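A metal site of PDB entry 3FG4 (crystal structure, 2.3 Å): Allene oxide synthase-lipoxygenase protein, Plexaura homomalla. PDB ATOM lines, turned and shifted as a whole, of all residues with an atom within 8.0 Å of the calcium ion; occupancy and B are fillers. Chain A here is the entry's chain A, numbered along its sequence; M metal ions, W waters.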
ATOM      1  N   THR A  15     -27.405   6.944  35.119  1.00  0.00           N
ATOM      2  CA  THR A  15     -26.641   6.136  34.216  1.00  0.00           C
ATOM      3  C   THR A  15     -25.648   5.178  34.916  1.00  0.00           C
ATOM      4  O   THR A  15     -24.952   5.534  35.872  1.00  0.00           O
ATOM      5  CB  THR A  15     -25.912   6.997  33.188  1.00  0.00           C
ATOM      6  OG1 THR A  15     -26.874   7.675  32.413  1.00  0.00           O
ATOM      7  CG2 THR A  15     -25.066   6.144  32.249  1.00  0.00           C
ATOM      8  N   ARG A  18     -20.663   1.327  34.414  1.00  0.00           N
ATOM      9  CA  ARG A  18     -19.832   0.502  33.564  1.00  0.00           C
ATOM     10  C   ARG A  18     -19.293   1.333  32.374  1.00  0.00           C
ATOM     11  O   ARG A  18     -19.867   2.334  31.971  1.00  0.00           O
ATOM     12  CB  ARG A  18     -20.591  -0.738  33.114  1.00  0.00           C
ATOM     13  CG  ARG A  18     -21.782  -0.518  32.155  1.00  0.00           C
ATOM     14  CD  ARG A  18     -22.592  -1.822  32.121  1.00  0.00           C
ATOM     15  NE  ARG A  18     -23.195  -2.017  33.469  1.00  0.00           N
ATOM     16  CZ  ARG A  18     -23.833  -3.114  33.894  1.00  0.00           C
ATOM     17  NH1 ARG A  18     -23.937  -4.135  33.056  1.00  0.00           N
ATOM     18  NH2 ARG A  18     -24.342  -3.151  35.134  1.00  0.00           N
ATOM     19  N   GLU A  19     -18.171   0.906  31.831  1.00  0.00           N
ATOM     20  CA  GLU A  19     -17.627   1.539  30.675  1.00  0.00           C
ATOM     21  C   GLU A  19     -18.591   1.512  29.523  1.00  0.00           C
ATOM     22  O   GLU A  19     -19.268   0.493  29.257  1.00  0.00           O
ATOM     23  CB  GLU A  19     -16.344   0.839  30.260  1.00  0.00           C
ATOM     24  CG  GLU A  19     -15.188   1.165  31.159  1.00  0.00           C
ATOM     25  CD  GLU A  19     -13.981   0.342  30.767  1.00  0.00           C
ATOM     26  OE1 GLU A  19     -13.039   0.226  31.588  1.00  0.00           O
ATOM     27  OE2 GLU A  19     -14.020  -0.211  29.620  1.00  0.00           O
ATOM     28  N   HIS A  20     -18.601   2.630  28.787  1.00  0.00           N
ATOM     29  CA  HIS A  20     -19.434   2.861  27.601  1.00  0.00           C
ATOM     30  C   HIS A  20     -20.882   2.957  27.906  1.00  0.00           C
ATOM     31  O   HIS A  20     -21.666   3.019  26.972  1.00  0.00           O
ATOM     32  CB  HIS A  20     -19.168   1.867  26.501  1.00  0.00           C
ATOM     33  CG  HIS A  20     -17.907   2.159  25.772  1.00  0.00           C
ATOM     34  ND1 HIS A  20     -17.628   3.419  25.266  1.00  0.00           N
ATOM     35  CD2 HIS A  20     -16.813   1.404  25.544  1.00  0.00           C
ATOM     36  CE1 HIS A  20     -16.421   3.412  24.722  1.00  0.00           C
ATOM     37  NE2 HIS A  20     -15.901   2.210  24.881  1.00  0.00           N
ATOM     38  N   ALA A  21     -21.218   3.036  29.203  1.00  0.00           N
ATOM     39  CA  ALA A  21     -22.587   3.238  29.677  1.00  0.00           C
ATOM     40  C   ALA A  21     -23.227   4.538  29.213  1.00  0.00           C
ATOM     41  O   ALA A  21     -24.475   4.616  29.109  1.00  0.00           O
ATOM     42  CB  ALA A  21     -22.620   3.225  31.255  1.00  0.00           C
ATOM     43  N   GLY A  22     -22.395   5.578  29.029  1.00  0.00           N
ATOM     44  CA  GLY A  22     -22.889   6.921  28.671  1.00  0.00           C
ATOM     45  C   GLY A  22     -23.367   6.999  27.239  1.00  0.00           C
ATOM     46  O   GLY A  22     -23.144   6.088  26.422  1.00  0.00           O
ATOM     47  N   THR A  23     -24.013   8.118  26.883  1.00  0.00           N
ATOM     48  CA  THR A  23     -24.373   8.331  25.481  1.00  0.00           C
ATOM     49  C   THR A  23     -24.329   9.801  25.131  1.00  0.00           C
ATOM     50  O   THR A  23     -24.431  10.609  26.016  1.00  0.00           O
ATOM     51  CB  THR A  23     -25.791   7.797  25.196  1.00  0.00           C
ATOM     52  OG1 THR A  23     -26.069   7.928  23.799  1.00  0.00           O
ATOM     53  CG2 THR A  23     -26.861   8.553  26.001  1.00  0.00           C
ATOM     54  N   ASP A  24     -24.191  10.133  23.835  1.00  0.00           N
ATOM     55  CA  ASP A  24     -24.498  11.469  23.336  1.00  0.00           C
ATOM     56  C   ASP A  24     -25.589  11.384  22.311  1.00  0.00           C
ATOM     57  O   ASP A  24     -25.773  12.320  21.542  1.00  0.00           O
ATOM     58  CB  ASP A  24     -23.277  12.169  22.737  1.00  0.00           C
ATOM     59  CG  ASP A  24     -22.671  11.405  21.572  1.00  0.00           C
ATOM     60  OD1 ASP A  24     -23.173  10.297  21.211  1.00  0.00           O
ATOM     61  OD2 ASP A  24     -21.662  11.904  21.023  1.00  0.00           O
ATOM     62  N   ALA A  25     -26.311  10.269  22.259  1.00  0.00           N
ATOM     63  CA  ALA A  25     -27.506  10.237  21.424  1.00  0.00           C
ATOM     64  C   ALA A  25     -28.412  11.323  21.946  1.00  0.00           C
ATOM     65  O   ALA A  25     -28.296  11.736  23.114  1.00  0.00           O
ATOM     66  CB  ALA A  25     -28.195   8.933  21.496  1.00  0.00           C
ATOM     67  N   PHE A  48     -24.835  12.710  29.446  1.00  0.00           N
ATOM     68  CA  PHE A  48     -25.129  11.421  29.995  1.00  0.00           C
ATOM     69  C   PHE A  48     -23.813  10.659  30.079  1.00  0.00           C
ATOM     70  O   PHE A  48     -23.530   9.874  29.222  1.00  0.00           O
ATOM     71  CB  PHE A  48     -26.157  10.716  29.093  1.00  0.00           C
ATOM     72  CG  PHE A  48     -27.580  11.182  29.344  1.00  0.00           C
ATOM     73  CD1 PHE A  48     -28.387  11.649  28.280  1.00  0.00           C
ATOM     74  CD2 PHE A  48     -28.110  11.205  30.649  1.00  0.00           C
ATOM     75  CE1 PHE A  48     -29.675  12.135  28.535  1.00  0.00           C
ATOM     76  CE2 PHE A  48     -29.399  11.662  30.888  1.00  0.00           C
ATOM     77  CZ  PHE A  48     -30.194  12.127  29.815  1.00  0.00           C
ATOM     78  N   ALA A  50     -21.209   7.950  32.043  1.00  0.00           N
ATOM     79  CA  ALA A  50     -21.215   6.795  32.992  1.00  0.00           C
ATOM     80  C   ALA A  50     -21.219   7.266  34.432  1.00  0.00           C
ATOM     81  O   ALA A  50     -20.527   8.243  34.771  1.00  0.00           O
ATOM     82  CB  ALA A  50     -20.028   5.777  32.716  1.00  0.00           C
ATOM     83  N   GLY A  81     -19.531   7.817  19.172  1.00  0.00           N
ATOM     84  CA  GLY A  81     -18.655   6.642  19.256  1.00  0.00           C
ATOM     85  C   GLY A  81     -19.460   5.416  19.636  1.00  0.00           C
ATOM     86  O   GLY A  81     -19.332   4.367  19.001  1.00  0.00           O
ATOM     87  N   ASP A  82     -20.301   5.555  20.677  1.00  0.00           N
ATOM     88  CA  ASP A  82     -21.060   4.422  21.265  1.00  0.00           C
ATOM     89  C   ASP A  82     -22.417   4.901  21.802  1.00  0.00           C
ATOM     90  O   ASP A  82     -22.557   5.158  23.000  1.00  0.00           O
ATOM     91  CB  ASP A  82     -20.227   3.725  22.329  1.00  0.00           C
ATOM     92  CG  ASP A  82     -20.918   2.485  22.886  1.00  0.00           C
ATOM     93  OD1 ASP A  82     -21.053   1.501  22.127  1.00  0.00           O
ATOM     94  OD2 ASP A  82     -21.381   2.501  24.060  1.00  0.00           O
ATOM     95  N   PRO A  83     -23.425   5.028  20.918  1.00  0.00           N
ATOM     96  CA  PRO A  83     -24.701   5.578  21.370  1.00  0.00           C
ATOM     97  C   PRO A  83     -25.476   4.749  22.414  1.00  0.00           C
ATOM     98  O   PRO A  83     -26.265   5.317  23.173  1.00  0.00           O
ATOM     99  CB  PRO A  83     -25.514   5.741  20.062  1.00  0.00           C
ATOM    100  CG  PRO A  83     -24.801   4.815  19.006  1.00  0.00           C
ATOM    101  CD  PRO A  83     -23.334   4.913  19.437  1.00  0.00           C
ATOM    102  N   ASP A  84     -25.312   3.425  22.425  1.00  0.00           N
ATOM    103  CA  ASP A  84     -25.961   2.607  23.452  1.00  0.00           C
ATOM    104  C   ASP A  84     -25.646   3.122  24.859  1.00  0.00           C
ATOM    105  O   ASP A  84     -24.522   3.465  25.191  1.00  0.00           O
ATOM    106  CB  ASP A  84     -25.524   1.145  23.366  1.00  0.00           C
ATOM    107  CG  ASP A  84     -25.827   0.491  21.990  1.00  0.00           C
ATOM    108  OD1 ASP A  84     -25.254  -0.597  21.771  1.00  0.00           O
ATOM    109  OD2 ASP A  84     -26.612   1.031  21.143  1.00  0.00           O
ATOM    110  N   TRP A  85     -26.671   3.108  25.692  1.00  0.00           N
ATOM    111  CA  TRP A  85     -26.733   3.855  26.924  1.00  0.00           C
ATOM    112  C   TRP A  85     -27.269   2.871  27.988  1.00  0.00           C
ATOM    113  O   TRP A  85     -28.365   2.355  27.818  1.00  0.00           O
ATOM    114  CB  TRP A  85     -27.754   4.978  26.692  1.00  0.00           C
ATOM    115  CG  TRP A  85     -28.038   5.893  27.796  1.00  0.00           C
ATOM    116  CD1 TRP A  85     -27.175   6.297  28.769  1.00  0.00           C
ATOM    117  CD2 TRP A  85     -29.289   6.607  28.042  1.00  0.00           C
ATOM    118  NE1 TRP A  85     -27.816   7.189  29.626  1.00  0.00           N
ATOM    119  CE2 TRP A  85     -29.100   7.414  29.188  1.00  0.00           C
ATOM    120  CE3 TRP A  85     -30.524   6.632  27.396  1.00  0.00           C
ATOM    121  CZ2 TRP A  85     -30.099   8.265  29.697  1.00  0.00           C
ATOM    122  CZ3 TRP A  85     -31.544   7.486  27.937  1.00  0.00           C
ATOM    123  CH2 TRP A  85     -31.303   8.277  29.082  1.00  0.00           C
ATOM    124  N   PHE A  86     -26.488   2.599  29.027  1.00  0.00           N
ATOM    125  CA  PHE A  86     -26.912   1.728  30.084  1.00  0.00           C
ATOM    126  C   PHE A  86     -27.556   2.538  31.193  1.00  0.00           C
ATOM    127  O   PHE A  86     -26.856   3.246  31.925  1.00  0.00           O
ATOM    128  CB  PHE A  86     -25.710   0.907  30.630  1.00  0.00           C
ATOM    129  CG  PHE A  86     -26.131  -0.211  31.567  1.00  0.00           C
ATOM    130  CD1 PHE A  86     -26.308  -1.502  31.091  1.00  0.00           C
ATOM    131  CD2 PHE A  86     -26.439   0.060  32.918  1.00  0.00           C
ATOM    132  CE1 PHE A  86     -26.746  -2.554  31.950  1.00  0.00           C
ATOM    133  CE2 PHE A  86     -26.850  -0.975  33.796  1.00  0.00           C
ATOM    134  CZ  PHE A  86     -26.989  -2.302  33.305  1.00  0.00           C
ATOM    135  N   TRP A 108     -29.366  -2.147  28.716  1.00  0.00           N
ATOM    136  CA  TRP A 108     -28.949  -1.286  27.652  1.00  0.00           C
ATOM    137  C   TRP A 108     -30.116  -0.672  26.849  1.00  0.00           C
ATOM    138  O   TRP A 108     -30.987  -1.363  26.356  1.00  0.00           O
ATOM    139  CB  TRP A 108     -28.020  -2.055  26.708  1.00  0.00           C
ATOM    140  CG  TRP A 108     -26.672  -2.279  27.352  1.00  0.00           C
ATOM    141  CD1 TRP A 108     -26.259  -3.393  28.054  1.00  0.00           C
ATOM    142  CD2 TRP A 108     -25.568  -1.347  27.417  1.00  0.00           C
ATOM    143  NE1 TRP A 108     -24.967  -3.210  28.558  1.00  0.00           N
ATOM    144  CE2 TRP A 108     -24.512  -1.972  28.162  1.00  0.00           C
ATOM    145  CE3 TRP A 108     -25.364  -0.042  26.910  1.00  0.00           C
ATOM    146  CZ2 TRP A 108     -23.298  -1.337  28.411  1.00  0.00           C
ATOM    147  CZ3 TRP A 108     -24.126   0.589  27.155  1.00  0.00           C
ATOM    148  CH2 TRP A 108     -23.129  -0.049  27.922  1.00  0.00           C
ATOM    149  N   VAL A 109     -30.080   0.638  26.680  1.00  0.00           N
ATOM    150  CA  VAL A 109     -30.995   1.336  25.799  1.00  0.00           C
ATOM    151  C   VAL A 109     -30.359   1.530  24.447  1.00  0.00           C
ATOM    152  O   VAL A 109     -29.370   2.236  24.310  1.00  0.00           O
ATOM    153  CB  VAL A 109     -31.400   2.695  26.403  1.00  0.00           C
ATOM    154  CG1 VAL A 109     -32.447   3.438  25.508  1.00  0.00           C
ATOM    155  CG2 VAL A 109     -31.976   2.418  27.755  1.00  0.00           C
ATOM    156  N   ARG A 169     -26.701  -6.833  23.641  1.00  0.00           N
ATOM    157  CA  ARG A 169     -25.756  -6.221  24.504  1.00  0.00           C
ATOM    158  C   ARG A 169     -26.005  -6.615  25.946  1.00  0.00           C
ATOM    159  O   ARG A 169     -25.023  -6.737  26.705  1.00  0.00           O
ATOM    160  CB  ARG A 169     -25.765  -4.695  24.315  1.00  0.00           C
ATOM    161  CG  ARG A 169     -24.436  -4.085  24.611  1.00  0.00           C
ATOM    162  CD  ARG A 169     -24.269  -2.669  24.025  1.00  0.00           C
ATOM    163  NE  ARG A 169     -23.060  -2.091  24.621  1.00  0.00           N
ATOM    164  CZ  ARG A 169     -22.322  -1.115  24.095  1.00  0.00           C
ATOM    165  NH1 ARG A 169     -22.644  -0.549  22.908  1.00  0.00           N
ATOM    166  NH2 ARG A 169     -21.252  -0.701  24.754  1.00  0.00           N
ATOM    167  N   ASP A 175     -17.320  -4.262  29.134  1.00  0.00           N
ATOM    168  CA  ASP A 175     -16.079  -3.934  28.475  1.00  0.00           C
ATOM    169  C   ASP A 175     -14.919  -4.208  29.441  1.00  0.00           C
ATOM    170  O   ASP A 175     -13.862  -4.747  29.055  1.00  0.00           O
ATOM    171  CB  ASP A 175     -16.125  -2.473  27.957  1.00  0.00           C
ATOM    172  CG  ASP A 175     -16.837  -2.351  26.589  1.00  0.00           C
ATOM    173  OD1 ASP A 175     -17.591  -1.400  26.371  1.00  0.00           O
ATOM    174  OD2 ASP A 175     -16.686  -3.239  25.712  1.00  0.00           O
HETATM  175 CA    CA M   1     -22.368   4.275  25.154  1.00  0.00          CA
HETATM  176  O   HOH W   1     -20.316   5.355  25.208  1.00  0.00           O
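Of the 21 residues printed, 4 come within 4 Å of the calcium ion.
The side-chain carboxylate of Asp 84 lies within salt-bridge range of the guanidinium group of Arg 169. The guanidinium group (NH1) of Arg 169 lies within salt-bridge range of the side-chain carboxylate (OD1) of Asp 82 (2.7 Å).
The calcium ion is bound by O of Asp 84, OD2 of Asp 82, water W1, O of His 20, O of Asp 82 and O of Gly 22.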
